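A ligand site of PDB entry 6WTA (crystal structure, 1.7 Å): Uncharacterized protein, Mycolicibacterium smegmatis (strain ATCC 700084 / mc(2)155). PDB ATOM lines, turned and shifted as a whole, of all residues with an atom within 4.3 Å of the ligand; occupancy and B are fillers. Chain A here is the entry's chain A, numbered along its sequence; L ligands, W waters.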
ATOM      1  N   SER A   7       8.056 -21.281 -22.599  1.00  0.00           N
ATOM      2  CA  SER A   7       7.328 -20.731 -23.722  1.00  0.00           C
ATOM      3  C   SER A   7       7.536 -21.608 -24.965  1.00  0.00           C
ATOM      4  O   SER A   7       8.650 -22.100 -25.196  1.00  0.00           O
ATOM      5  CB  SER A   7       7.788 -19.308 -24.015  1.00  0.00           C
ATOM      6  OG  SER A   7       7.148 -18.800 -25.178  1.00  0.00           O
ATOM      7  N   PRO A   8       6.499 -21.807 -25.782  1.00  0.00           N
ATOM      8  CA  PRO A   8       6.737 -22.434 -27.096  1.00  0.00           C
ATOM      9  C   PRO A   8       7.498 -21.518 -28.043  1.00  0.00           C
ATOM     10  O   PRO A   8       8.036 -22.009 -29.046  1.00  0.00           O
ATOM     11  CB  PRO A   8       5.324 -22.721 -27.609  1.00  0.00           C
ATOM     12  CG  PRO A   8       4.472 -21.663 -26.970  1.00  0.00           C
ATOM     13  CD  PRO A   8       5.089 -21.440 -25.586  1.00  0.00           C
ATOM     14  N   THR A   9       7.573 -20.227 -27.761  1.00  0.00           N
ATOM     15  CA  THR A   9       8.292 -19.276 -28.608  1.00  0.00           C
ATOM     16  C   THR A   9       9.791 -19.396 -28.360  1.00  0.00           C
ATOM     17  O   THR A   9      10.246 -19.273 -27.228  1.00  0.00           O
ATOM     18  CB  THR A   9       7.806 -17.857 -28.343  1.00  0.00           C
ATOM     19  OG1 THR A   9       6.383 -17.803 -28.465  1.00  0.00           O
ATOM     20  CG2 THR A   9       8.429 -16.880 -29.334  1.00  0.00           C
ATOM     21  N   TRP A  11      12.717 -17.726 -28.940  1.00  0.00           N
ATOM     22  CA  TRP A  11      13.577 -16.734 -28.289  1.00  0.00           C
ATOM     23  C   TRP A  11      13.138 -16.490 -26.843  1.00  0.00           C
ATOM     24  O   TRP A  11      13.990 -16.224 -25.988  1.00  0.00           O
ATOM     25  CB  TRP A  11      13.588 -15.426 -29.078  1.00  0.00           C
ATOM     26  CG  TRP A  11      12.357 -14.571 -28.971  1.00  0.00           C
ATOM     27  CD1 TRP A  11      11.222 -14.680 -29.716  1.00  0.00           C
ATOM     28  CD2 TRP A  11      12.156 -13.460 -28.088  1.00  0.00           C
ATOM     29  NE1 TRP A  11      10.316 -13.723 -29.349  1.00  0.00           N
ATOM     30  CE2 TRP A  11      10.868 -12.955 -28.342  1.00  0.00           C
ATOM     31  CE3 TRP A  11      12.935 -12.847 -27.101  1.00  0.00           C
ATOM     32  CZ2 TRP A  11      10.333 -11.865 -27.660  1.00  0.00           C
ATOM     33  CZ3 TRP A  11      12.406 -11.766 -26.416  1.00  0.00           C
ATOM     34  CH2 TRP A  11      11.124 -11.287 -26.696  1.00  0.00           C
ATOM     35  N   VAL A  12      11.838 -16.583 -26.563  1.00  0.00           N
ATOM     36  CA  VAL A  12      11.366 -16.426 -25.193  1.00  0.00           C
ATOM     37  C   VAL A  12      11.823 -17.606 -24.337  1.00  0.00           C
ATOM     38  O   VAL A  12      12.281 -17.432 -23.201  1.00  0.00           O
ATOM     39  CB  VAL A  12       9.842 -16.272 -25.152  1.00  0.00           C
ATOM     40  CG1 VAL A  12       9.361 -16.055 -23.711  1.00  0.00           C
ATOM     41  CG2 VAL A  12       9.380 -15.154 -26.052  1.00  0.00           C
ATOM     42  N   GLN A  15      15.563 -17.229 -23.600  1.00  0.00           N
ATOM     43  CA  GLN A  15      15.862 -16.268 -22.554  1.00  0.00           C
ATOM     44  C   GLN A  15      15.454 -16.788 -21.189  1.00  0.00           C
ATOM     45  O   GLN A  15      16.153 -16.564 -20.191  1.00  0.00           O
ATOM     46  CB  GLN A  15      15.182 -14.926 -22.848  1.00  0.00           C
ATOM     47  CG  GLN A  15      15.841 -14.140 -23.979  1.00  0.00           C
ATOM     48  CD  GLN A  15      15.628 -12.644 -23.861  1.00  0.00           C
ATOM     49  OE1 GLN A  15      16.548 -11.863 -24.103  1.00  0.00           O
ATOM     50  NE2 GLN A  15      14.423 -12.234 -23.501  1.00  0.00           N
ATOM     51  N   VAL A  30      16.273  -7.211 -23.429  1.00  0.00           N
ATOM     52  CA  VAL A  30      15.610  -6.919 -24.688  1.00  0.00           C
ATOM     53  C   VAL A  30      15.903  -5.465 -25.037  1.00  0.00           C
ATOM     54  O   VAL A  30      15.652  -4.568 -24.225  1.00  0.00           O
ATOM     55  CB  VAL A  30      14.091  -7.180 -24.608  1.00  0.00           C
ATOM     56  CG1 VAL A  30      13.380  -6.516 -25.786  1.00  0.00           C
ATOM     57  CG2 VAL A  30      13.807  -8.674 -24.591  1.00  0.00           C
ATOM     58  N   ILE A  35      14.692  -7.124 -17.806  1.00  0.00           N
ATOM     59  CA  ILE A  35      13.453  -7.885 -17.820  1.00  0.00           C
ATOM     60  C   ILE A  35      13.276  -8.568 -16.472  1.00  0.00           C
ATOM     61  O   ILE A  35      14.208  -8.710 -15.678  1.00  0.00           O
ATOM     62  CB  ILE A  35      13.432  -8.941 -18.956  1.00  0.00           C
ATOM     63  CG1 ILE A  35      14.426 -10.064 -18.668  1.00  0.00           C
ATOM     64  CG2 ILE A  35      13.747  -8.292 -20.295  1.00  0.00           C
ATOM     65  CD1 ILE A  35      14.388 -11.186 -19.695  1.00  0.00           C
ATOM     66  N   GLY A  42      -2.025 -21.150 -15.926  1.00  0.00           N
ATOM     67  CA  GLY A  42      -2.894 -21.132 -17.081  1.00  0.00           C
ATOM     68  C   GLY A  42      -4.349 -21.294 -16.706  1.00  0.00           C
ATOM     69  O   GLY A  42      -4.717 -22.124 -15.875  1.00  0.00           O
ATOM     70  N   ALA A  43      -5.207 -20.490 -17.356  1.00  0.00           N
ATOM     71  CA  ALA A  43      -6.608 -20.436 -16.960  1.00  0.00           C
ATOM     72  C   ALA A  43      -7.299 -21.773 -17.152  1.00  0.00           C
ATOM     73  O   ALA A  43      -8.163 -22.156 -16.351  1.00  0.00           O
ATOM     74  CB  ALA A  43      -7.330 -19.351 -17.758  1.00  0.00           C
ATOM     75  N   LYS A  44      -6.936 -22.509 -18.203  1.00  0.00           N
ATOM     76  CA  LYS A  44      -7.582 -23.792 -18.476  1.00  0.00           C
ATOM     77  C   LYS A  44      -6.747 -24.984 -18.042  1.00  0.00           C
ATOM     78  O   LYS A  44      -7.294 -25.970 -17.550  1.00  0.00           O
ATOM     79  CB  LYS A  44      -7.899 -23.911 -19.963  1.00  0.00           C
ATOM     80  CG  LYS A  44      -8.994 -22.978 -20.438  1.00  0.00           C
ATOM     81  CD  LYS A  44      -8.551 -22.227 -21.675  1.00  0.00           C
ATOM     82  CE  LYS A  44      -9.039 -22.926 -22.937  1.00  0.00           C
ATOM     83  NZ  LYS A  44     -10.436 -22.523 -23.247  1.00  0.00           N
ATOM     84  N   SER A  45      -5.425 -24.924 -18.222  1.00  0.00           N
ATOM     85  CA  SER A  45      -4.589 -26.062 -17.908  1.00  0.00           C
ATOM     86  C   SER A  45      -4.253 -26.162 -16.438  1.00  0.00           C
ATOM     87  O   SER A  45      -3.956 -27.255 -15.951  1.00  0.00           O
ATOM     88  CB  SER A  45      -3.283 -25.976 -18.710  1.00  0.00           C
ATOM     89  OG  SER A  45      -2.485 -24.913 -18.245  1.00  0.00           O
ATOM     90  N   ARG A  49       3.310 -21.323 -15.797  1.00  0.00           N
ATOM     91  CA  ARG A  49       3.976 -20.878 -17.022  1.00  0.00           C
ATOM     92  C   ARG A  49       4.900 -19.708 -16.714  1.00  0.00           C
ATOM     93  O   ARG A  49       4.506 -18.750 -16.038  1.00  0.00           O
ATOM     94  CB  ARG A  49       2.965 -20.470 -18.084  1.00  0.00           C
ATOM     95  CG  ARG A  49       2.037 -21.603 -18.471  1.00  0.00           C
ATOM     96  CD  ARG A  49       1.268 -21.291 -19.732  1.00  0.00           C
ATOM     97  NE  ARG A  49       0.310 -22.345 -20.064  1.00  0.00           N
ATOM     98  CZ  ARG A  49       0.640 -23.503 -20.629  1.00  0.00           C
ATOM     99  NH1 ARG A  49       1.903 -23.768 -20.927  1.00  0.00           N
ATOM    100  NH2 ARG A  49      -0.307 -24.392 -20.900  1.00  0.00           N
ATOM    101  N   VAL A  51       6.689 -16.469 -17.743  1.00  0.00           N
ATOM    102  CA  VAL A  51       6.481 -15.375 -18.675  1.00  0.00           C
ATOM    103  C   VAL A  51       7.465 -14.243 -18.380  1.00  0.00           C
ATOM    104  O   VAL A  51       7.255 -13.495 -17.406  1.00  0.00           O
ATOM    105  CB  VAL A  51       5.034 -14.851 -18.621  1.00  0.00           C
ATOM    106  CG1 VAL A  51       4.830 -13.714 -19.631  1.00  0.00           C
ATOM    107  CG2 VAL A  51       4.041 -15.975 -18.867  1.00  0.00           C
ATOM    108  N   PRO A  52       8.528 -14.092 -19.153  1.00  0.00           N
ATOM    109  CA  PRO A  52       9.367 -12.894 -19.008  1.00  0.00           C
ATOM    110  C   PRO A  52       8.666 -11.684 -19.594  1.00  0.00           C
ATOM    111  O   PRO A  52       7.977 -11.788 -20.617  1.00  0.00           O
ATOM    112  CB  PRO A  52      10.644 -13.240 -19.805  1.00  0.00           C
ATOM    113  CG  PRO A  52      10.495 -14.673 -20.243  1.00  0.00           C
ATOM    114  CD  PRO A  52       9.038 -15.012 -20.192  1.00  0.00           C
ATOM    115  N   LEU A  53       8.818 -10.539 -18.939  1.00  0.00           N
ATOM    116  CA  LEU A  53       8.284  -9.273 -19.411  1.00  0.00           C
ATOM    117  C   LEU A  53       9.305  -8.181 -19.124  1.00  0.00           C
ATOM    118  O   LEU A  53      10.250  -8.380 -18.350  1.00  0.00           O
ATOM    119  CB  LEU A  53       6.962  -8.933 -18.724  1.00  0.00           C
ATOM    120  CG  LEU A  53       5.790  -9.884 -18.944  1.00  0.00           C
ATOM    121  CD1 LEU A  53       4.589  -9.438 -18.117  1.00  0.00           C
ATOM    122  CD2 LEU A  53       5.439  -9.971 -20.412  1.00  0.00           C
ATOM    123  N   MET A  54       9.130  -7.016 -19.753  1.00  0.00           N
ATOM    124  CA  MET A  54      10.024  -5.912 -19.450  1.00  0.00           C
ATOM    125  C   MET A  54       9.864  -5.511 -17.987  1.00  0.00           C
ATOM    126  O   MET A  54       8.780  -5.616 -17.409  1.00  0.00           O
ATOM    127  CB  MET A  54       9.738  -4.699 -20.342  1.00  0.00           C
ATOM    128  CG  MET A  54       9.890  -4.947 -21.839  1.00  0.00           C
ATOM    129  SD  MET A  54      11.384  -5.826 -22.336  1.00  0.00           S
ATOM    130  CE  MET A  54      12.663  -4.746 -21.704  1.00  0.00           C
ATOM    131  N   VAL A  65       2.835  -5.478 -18.854  1.00  0.00           N
ATOM    132  CA  VAL A  65       2.263  -4.758 -19.994  1.00  0.00           C
ATOM    133  C   VAL A  65       2.016  -5.755 -21.118  1.00  0.00           C
ATOM    134  O   VAL A  65       2.962  -6.350 -21.652  1.00  0.00           O
ATOM    135  CB  VAL A  65       3.178  -3.609 -20.464  1.00  0.00           C
ATOM    136  CG1 VAL A  65       2.539  -2.905 -21.654  1.00  0.00           C
ATOM    137  CG2 VAL A  65       3.430  -2.641 -19.324  1.00  0.00           C
ATOM    138  N   ALA A  66       0.752  -5.900 -21.511  1.00  0.00           N
ATOM    139  CA  ALA A  66       0.343  -6.974 -22.418  1.00  0.00           C
ATOM    140  C   ALA A  66       0.340  -6.481 -23.863  1.00  0.00           C
ATOM    141  O   ALA A  66      -0.695  -6.129 -24.429  1.00  0.00           O
ATOM    142  CB  ALA A  66      -1.022  -7.515 -22.013  1.00  0.00           C
ATOM    143  N   SER A  67       1.517  -6.483 -24.471  1.00  0.00           N
ATOM    144  CA  SER A  67       1.646  -6.078 -25.870  1.00  0.00           C
ATOM    145  C   SER A  67       2.769  -6.888 -26.495  1.00  0.00           C
ATOM    146  O   SER A  67       3.943  -6.510 -26.429  1.00  0.00           O
ATOM    147  CB  SER A  67       1.892  -4.583 -25.987  1.00  0.00           C
ATOM    148  OG  SER A  67       3.137  -4.225 -25.412  1.00  0.00           O
ATOM    149  N   LYS A  68       2.408  -8.027 -27.107  1.00  0.00           N
ATOM    150  CA  LYS A  68       3.387  -8.885 -27.772  1.00  0.00           C
ATOM    151  C   LYS A  68       3.778  -8.263 -29.114  1.00  0.00           C
ATOM    152  O   LYS A  68       3.460  -8.769 -30.197  1.00  0.00           O
ATOM    153  CB  LYS A  68       2.834 -10.298 -27.928  1.00  0.00           C
ATOM    154  CG  LYS A  68       1.419 -10.388 -28.459  1.00  0.00           C
ATOM    155  CD  LYS A  68       0.973 -11.846 -28.579  1.00  0.00           C
ATOM    156  CE  LYS A  68      -0.482 -11.939 -29.024  1.00  0.00           C
ATOM    157  NZ  LYS A  68      -0.960 -13.350 -29.115  1.00  0.00           N
ATOM    158  N   HIS A  74      -4.717 -10.118 -27.587  1.00  0.00           N
ATOM    159  CA  HIS A  74      -4.164 -10.264 -26.245  1.00  0.00           C
ATOM    160  C   HIS A  74      -3.312 -11.526 -26.178  1.00  0.00           C
ATOM    161  O   HIS A  74      -3.686 -12.554 -26.746  1.00  0.00           O
ATOM    162  CB  HIS A  74      -5.256 -10.336 -25.181  1.00  0.00           C
ATOM    163  CG  HIS A  74      -6.094  -9.106 -25.076  1.00  0.00           C
ATOM    164  ND1 HIS A  74      -5.554  -7.849 -24.891  1.00  0.00           N
ATOM    165  CD2 HIS A  74      -7.442  -8.938 -25.109  1.00  0.00           C
ATOM    166  CE1 HIS A  74      -6.530  -6.960 -24.824  1.00  0.00           C
ATOM    167  NE2 HIS A  74      -7.684  -7.592 -24.954  1.00  0.00           N
ATOM    168  N   PRO A  75      -2.180 -11.500 -25.474  1.00  0.00           N
ATOM    169  CA  PRO A  75      -1.443 -12.737 -25.226  1.00  0.00           C
ATOM    170  C   PRO A  75      -2.203 -13.638 -24.271  1.00  0.00           C
ATOM    171  O   PRO A  75      -3.044 -13.193 -23.491  1.00  0.00           O
ATOM    172  CB  PRO A  75      -0.117 -12.265 -24.622  1.00  0.00           C
ATOM    173  CG  PRO A  75      -0.477 -10.983 -23.915  1.00  0.00           C
ATOM    174  CD  PRO A  75      -1.544 -10.339 -24.806  1.00  0.00           C
ATOM    175  N   SER A  76      -1.904 -14.934 -24.361  1.00  0.00           N
ATOM    176  CA  SER A  76      -2.577 -15.887 -23.486  1.00  0.00           C
ATOM    177  C   SER A  76      -2.373 -15.542 -22.020  1.00  0.00           C
ATOM    178  O   SER A  76      -3.286 -15.714 -21.206  1.00  0.00           O
ATOM    179  CB  SER A  76      -2.076 -17.306 -23.788  1.00  0.00           C
ATOM    180  OG  SER A  76      -2.542 -17.754 -25.051  1.00  0.00           O
ATOM    181  N   TRP A  77      -1.188 -15.035 -21.652  1.00  0.00           N
ATOM    182  CA  TRP A  77      -0.945 -14.765 -20.240  1.00  0.00           C
ATOM    183  C   TRP A  77      -1.865 -13.677 -19.699  1.00  0.00           C
ATOM    184  O   TRP A  77      -2.088 -13.613 -18.487  1.00  0.00           O
ATOM    185  CB  TRP A  77       0.530 -14.403 -20.004  1.00  0.00           C
ATOM    186  CG  TRP A  77       1.053 -13.118 -20.574  1.00  0.00           C
ATOM    187  CD1 TRP A  77       1.803 -12.979 -21.700  1.00  0.00           C
ATOM    188  CD2 TRP A  77       0.916 -11.812 -20.015  1.00  0.00           C
ATOM    189  NE1 TRP A  77       2.141 -11.661 -21.887  1.00  0.00           N
ATOM    190  CE2 TRP A  77       1.601 -10.919 -20.870  1.00  0.00           C
ATOM    191  CE3 TRP A  77       0.286 -11.307 -18.877  1.00  0.00           C
ATOM    192  CZ2 TRP A  77       1.663  -9.546 -20.612  1.00  0.00           C
ATOM    193  CZ3 TRP A  77       0.347  -9.949 -18.628  1.00  0.00           C
ATOM    194  CH2 TRP A  77       1.026  -9.085 -19.490  1.00  0.00           C
ATOM    195  N   PHE A  79      -5.165 -13.549 -20.264  1.00  0.00           N
ATOM    196  CA  PHE A  79      -6.312 -14.290 -19.751  1.00  0.00           C
ATOM    197  C   PHE A  79      -5.938 -15.104 -18.521  1.00  0.00           C
ATOM    198  O   PHE A  79      -6.752 -15.261 -17.599  1.00  0.00           O
ATOM    199  CB  PHE A  79      -6.870 -15.189 -20.843  1.00  0.00           C
ATOM    200  CG  PHE A  79      -7.246 -14.443 -22.105  1.00  0.00           C
ATOM    201  CD1 PHE A  79      -8.462 -13.794 -22.191  1.00  0.00           C
ATOM    202  CD2 PHE A  79      -6.386 -14.394 -23.187  1.00  0.00           C
ATOM    203  CE1 PHE A  79      -8.816 -13.101 -23.339  1.00  0.00           C
ATOM    204  CE2 PHE A  79      -6.726 -13.704 -24.332  1.00  0.00           C
ATOM    205  CZ  PHE A  79      -7.952 -13.059 -24.410  1.00  0.00           C
ATOM    206  N   ASN A  80      -4.687 -15.597 -18.460  1.00  0.00           N
ATOM    207  CA  ASN A  80      -4.254 -16.414 -17.332  1.00  0.00           C
ATOM    208  C   ASN A  80      -4.210 -15.591 -16.045  1.00  0.00           C
ATOM    209  O   ASN A  80      -4.646 -16.059 -14.980  1.00  0.00           O
ATOM    210  CB  ASN A  80      -2.883 -17.029 -17.622  1.00  0.00           C
ATOM    211  CG  ASN A  80      -2.937 -18.053 -18.738  1.00  0.00           C
ATOM    212  OD1 ASN A  80      -3.994 -18.587 -19.038  1.00  0.00           O
ATOM    213  ND2 ASN A  80      -1.792 -18.352 -19.319  1.00  0.00           N
ATOM    214  N   TYR A 123       7.103   0.453 -26.169  1.00  0.00           N
ATOM    215  CA  TYR A 123       5.703   0.331 -25.769  1.00  0.00           C
ATOM    216  C   TYR A 123       4.846   1.404 -26.436  1.00  0.00           C
ATOM    217  O   TYR A 123       3.705   1.155 -26.823  1.00  0.00           O
ATOM    218  CB  TYR A 123       5.535   0.431 -24.254  1.00  0.00           C
ATOM    219  CG  TYR A 123       5.817  -0.819 -23.451  1.00  0.00           C
ATOM    220  CD1 TYR A 123       5.460  -2.084 -23.910  1.00  0.00           C
ATOM    221  CD2 TYR A 123       6.433  -0.727 -22.213  1.00  0.00           C
ATOM    222  CE1 TYR A 123       5.727  -3.209 -23.148  1.00  0.00           C
ATOM    223  CE2 TYR A 123       6.698  -1.846 -21.462  1.00  0.00           C
ATOM    224  CZ  TYR A 123       6.348  -3.083 -21.924  1.00  0.00           C
ATOM    225  OH  TYR A 123       6.617  -4.193 -21.153  1.00  0.00           O
ATOM    226  N   ARG A 132      -7.245   0.322 -29.191  1.00  0.00           N
ATOM    227  CA  ARG A 132      -7.564   0.165 -27.779  1.00  0.00           C
ATOM    228  C   ARG A 132      -6.311   0.414 -26.941  1.00  0.00           C
ATOM    229  O   ARG A 132      -5.185   0.184 -27.392  1.00  0.00           O
ATOM    230  CB  ARG A 132      -8.101  -1.246 -27.491  1.00  0.00           C
ATOM    231  CG  ARG A 132      -9.602  -1.420 -27.677  1.00  0.00           C
ATOM    232  CD  ARG A 132     -10.036  -2.864 -27.386  1.00  0.00           C
ATOM    233  NE  ARG A 132      -9.553  -3.349 -26.091  1.00  0.00           N
ATOM    234  CZ  ARG A 132      -9.765  -4.569 -25.617  1.00  0.00           C
ATOM    235  NH1 ARG A 132     -10.448  -5.458 -26.322  1.00  0.00           N
ATOM    236  NH2 ARG A 132      -9.277  -4.911 -24.433  1.00  0.00           N
HETATM  237  C1  LIG L   1       6.450  -7.565 -22.746  1.00  0.00           C
HETATM  238  C2  LIG L   1      11.668 -10.845 -22.833  1.00  0.00           C
HETATM  239  C3  LIG L   1      10.908  -9.745 -22.573  1.00  0.00           C
HETATM  240  C4  LIG L   1       9.495  -9.734 -22.892  1.00  0.00           C
HETATM  241  C5  LIG L   1       8.928 -10.890 -23.466  1.00  0.00           C
HETATM  242  C6  LIG L   1       9.746 -12.010 -23.703  1.00  0.00           C
HETATM  243  C7  LIG L   1      11.089 -11.981 -23.392  1.00  0.00           C
HETATM  244  C8  LIG L   1       6.773  -9.807 -23.539  1.00  0.00           C
HETATM  245  C9  LIG L   1       4.671  -8.843 -23.646  1.00  0.00           C
HETATM  246  C10 LIG L   1       7.326  -8.648 -22.967  1.00  0.00           C
HETATM  247  C11 LIG L   1       8.677  -8.614 -22.655  1.00  0.00           C
HETATM  248  C12 LIG L   1       6.866 -12.051 -24.373  1.00  0.00           C
HETATM  249  C13 LIG L   1       6.118 -12.954 -23.405  1.00  0.00           C
HETATM  250  C14 LIG L   1       5.177 -13.867 -24.215  1.00  0.00           C
HETATM  251  C15 LIG L   1       4.184 -13.062 -25.064  1.00  0.00           C
HETATM  252  C16 LIG L   1       3.077 -13.962 -25.567  1.00  0.00           C
HETATM  253  C17 LIG L   1       3.120 -17.997 -27.315  1.00  0.00           C
HETATM  254  C18 LIG L   1       0.745 -22.432 -25.637  1.00  0.00           C
HETATM  255  C19 LIG L   1       1.223 -21.280 -24.729  1.00  0.00           C
HETATM  256  C20 LIG L   1       0.366 -21.226 -23.476  1.00  0.00           C
HETATM  257  C21 LIG L   1      -1.046 -20.765 -23.756  1.00  0.00           C
HETATM  258  C22 LIG L   1      -1.791 -20.654 -22.450  1.00  0.00           C
HETATM  259  C23 LIG L   1       2.208 -19.155 -25.314  1.00  0.00           C
HETATM  260  C24 LIG L   1       2.176 -17.889 -26.116  1.00  0.00           C
HETATM  261  C25 LIG L   1      -3.683 -22.332 -20.399  1.00  0.00           C
HETATM  262  C26 LIG L   1      -3.901 -21.061 -21.266  1.00  0.00           C
HETATM  263  C27 LIG L   1      -5.365 -20.781 -21.673  1.00  0.00           C
HETATM  264  C28 LIG L   1      -5.562 -19.338 -22.140  1.00  0.00           C
HETATM  265  C29 LIG L   1      -7.008 -18.871 -22.222  1.00  0.00           C
HETATM  266  C30 LIG L   1      -9.681 -18.917 -23.685  1.00  0.00           C
HETATM  267  C31 LIG L   1      -8.684 -17.735 -23.600  1.00  0.00           C
HETATM  268  C32 LIG L   1      -8.777 -16.910 -24.884  1.00  0.00           C
HETATM  269  C33 LIG L   1     -10.112 -16.197 -25.001  1.00  0.00           C
HETATM  270  C34 LIG L   1     -10.212 -15.312 -26.223  1.00  0.00           C
HETATM  271  C35 LIG L   1     -11.412 -13.858 -28.504  1.00  0.00           C
HETATM  272  C36 LIG L   1     -11.446 -13.252 -27.088  1.00  0.00           C
HETATM  273  C37 LIG L   1     -10.591 -11.979 -26.970  1.00  0.00           C
HETATM  274  C38 LIG L   1     -11.311 -10.759 -26.423  1.00  0.00           C
HETATM  275  C39 LIG L   1     -11.058 -10.377 -24.964  1.00  0.00           C
HETATM  276  N1  LIG L   1       7.558 -10.896 -23.765  1.00  0.00           N
HETATM  277  N2  LIG L   1       5.462  -9.867 -23.860  1.00  0.00           N
HETATM  278  N3  LIG L   1       5.122  -7.689 -23.092  1.00  0.00           N
HETATM  279  N4  LIG L   1       1.219 -20.030 -25.472  1.00  0.00           N
HETATM  280  N5  LIG L   1      -3.039 -21.095 -22.449  1.00  0.00           N
HETATM  281  N6  LIG L   1      -7.352 -18.237 -23.339  1.00  0.00           N
HETATM  282  N7  LIG L   1     -11.090 -14.284 -26.117  1.00  0.00           N
HETATM  283  O1  LIG L   1      11.832 -13.092 -23.653  1.00  0.00           O
HETATM  284  O2  LIG L   1       3.494  -8.952 -23.957  1.00  0.00           O
HETATM  285  O3  LIG L   1       6.893  -6.540 -22.258  1.00  0.00           O
HETATM  286  O4  LIG L   1       7.135 -13.576 -22.640  1.00  0.00           O
HETATM  287  O5  LIG L   1       5.912 -14.710 -25.142  1.00  0.00           O
HETATM  288  O6  LIG L   1       3.627 -11.915 -24.384  1.00  0.00           O
HETATM  289  O7  LIG L   1       2.418 -14.557 -24.432  1.00  0.00           O
HETATM  290  O8  LIG L   1       1.070 -16.197 -23.284  1.00  0.00           O
HETATM  291  O9  LIG L   1       0.506 -15.534 -25.768  1.00  0.00           O
HETATM  292  O10 LIG L   1       0.859 -23.585 -25.196  1.00  0.00           O
HETATM  293  O11 LIG L   1       0.275 -22.131 -26.750  1.00  0.00           O
HETATM  294  O12 LIG L   1       3.143 -19.358 -24.531  1.00  0.00           O
HETATM  295  O13 LIG L   1      -1.265 -20.187 -21.446  1.00  0.00           O
HETATM  296  O14 LIG L   1       2.588 -16.851 -25.266  1.00  0.00           O
HETATM  297  O15 LIG L   1      -2.634 -22.977 -20.569  1.00  0.00           O
HETATM  298  O16 LIG L   1      -4.566 -22.628 -19.583  1.00  0.00           O
HETATM  299  O17 LIG L   1      -7.820 -19.067 -21.315  1.00  0.00           O
HETATM  300  O18 LIG L   1     -10.763 -18.843 -23.060  1.00  0.00           O
HETATM  301  O19 LIG L   1      -9.321 -19.875 -24.376  1.00  0.00           O
HETATM  302  O20 LIG L   1      -9.523 -15.555 -27.213  1.00  0.00           O
HETATM  303  O21 LIG L   1     -12.247 -14.739 -28.766  1.00  0.00           O
HETATM  304  O22 LIG L   1     -10.549 -13.436 -29.290  1.00  0.00           O
HETATM  305  O23 LIG L   1     -11.418 -11.190 -24.082  1.00  0.00           O
HETATM  306  O24 LIG L   1     -10.510  -9.277 -24.713  1.00  0.00           O
HETATM  307  P1  LIG L   1       1.506 -15.850 -24.691  1.00  0.00           P
HETATM  308  O   HOH W   1       0.713 -15.154 -28.217  1.00  0.00           O
HETATM  309  O   HOH W   2       5.840 -15.161 -27.831  1.00  0.00           O
HETATM  310  O   HOH W   3      -6.795 -20.161 -25.704  1.00  0.00           O
HETATM  311  O   HOH W   4       3.393 -19.690 -22.120  1.00  0.00           O
HETATM  312  O   HOH W   5      -2.816 -21.260 -27.259  1.00  0.00           O
HETATM  313  O   HOH W   6      -5.345 -17.551 -25.259  1.00  0.00           O
HETATM  314  O   HOH W   7       1.582 -17.914 -21.377  1.00  0.00           O
HETATM  315  O   HOH W   8       5.405 -17.281 -24.099  1.00  0.00           O
HETATM  316  O   HOH W   9      -6.917 -15.537 -27.605  1.00  0.00           O
HETATM  317  O   HOH W  10      -1.123 -19.103 -27.064  1.00  0.00           O
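The backbone NH (N) of Ala 43 lies within hydrogen-bond range of an oxygen (O16) of the ligand. The guanidinium group (NH2) of Arg 49 lies within salt-bridge range of an oxygen (O15) of the ligand (2.7 Å). N of Ser 45 sits at hydrogen-bond distance from O16 of the ligand (2.8 Å). The backbone NH (N) of Ser 76 sits at hydrogen-bond distance from an oxygen (O9) of the ligand (2.9 Å). N of Lys 44 sits at hydrogen-bond distance from O16 of the ligand, 2.7 Å away. NE2 of Gln 15 is in hydrogen-bond range of O1 of the ligand (2.7 Å). N of Met 54 sits close to O3 of the ligand, 3.4 Å away. The side-chain amino group (NZ) of Lys 44 lies within salt-bridge range of an oxygen (O19) of the ligand (3.1 Å). An oxygen (O13) of the ligand sits at hydrogen-bond distance from the side-chain amide nitrogen (ND2) of Asn 80, 2.9 Å away. An oxygen (O2) of the ligand is in hydrogen-bond range of the backbone NH (N) of Ser 67, 3.2 Å away. An oxygen (O8) of the ligand lies within hydrogen-bond range of the backbone NH (N) of Trp 77. The backbone NH (N) of Lys 68 is in hydrogen-bond range of an oxygen (O2) of the ligand (3.5 Å). O of Pro 52 is in hydrogen-bond range of O4 of the ligand (2.8 Å). The side-chain hydroxyl (OH) of Tyr 123 is in hydrogen-bond range of an oxygen (O3) of the ligand, at 2.6 Å. OG of Ser 45 is in hydrogen-bond range of O15 of the ligand (3.0 Å). O of Val 65 is in hydrogen-bond range of N3 of the ligand (2.9 Å). An oxygen (O24) of the ligand sits close to a ring nitrogen (NE2) of His 74, 3.3 Å away. O6 of the ligand lies within hydrogen-bond range of NE1 of Trp 77 (2.9 Å).
The guanidinium group (NH2) of Arg 49 sits at hydrogen-bond distance from the side-chain hydroxyl (OG) of Ser 45, 3.5 Å away. NH2 of Arg 132 lies within hydrogen-bond range of NE2 of His 74 (3.2 Å). The backbone NH (N) of Thr 9 sits at hydrogen-bond distance from the side-chain hydroxyl (OG) of Ser 7 (3.0 Å). The side-chain amide oxygen (OD1) of Asn 80 is in hydrogen-bond range of the backbone NH (N) of Ala 43, at 2.8 Å.
Residues that only touch the ligand: Pro 8, Thr 9, Trp 11, Val 12, Val 30, Ile 35, Gly 42, Val 51, Leu 53, Pro 75 and Phe 79. 26 residues have an atom within 4 Å of the ligand: Pro 8, Thr 9, Trp 11, Val 12, Gln 15, Val 30, Ile 35, Gly 42, Ala 43, Lys 44, Ser 45, Arg 49, Val 51, Pro 52, Leu 53, Met 54, Val 65, Ser 67, Lys 68, His 74, Pro 75, Ser 76, Trp 77, Phe 79, Asn 80 and Tyr 123.
Water W1 bridges an oxygen (O9) of the ligand and the side-chain amino group (NZ) of Lys 68. Water W2 bridges an oxygen (O5) of the ligand (2.7 Å) and the side-chain hydroxyl of Thr 9 (2.8 Å). Water W8 lies within hydrogen-bond range of OG of Ser 7 (2.6 Å) and O5 of the ligand (2.8 Å). Water W6 bridges OG of Ser 76 (2.8 Å) and N6 of the ligand (2.9 Å). Water W10 lies within hydrogen-bond range of the side-chain hydroxyl (OG) of Ser 76 (2.8 Å) and a nitrogen (N4) of the ligand (3.0 Å).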
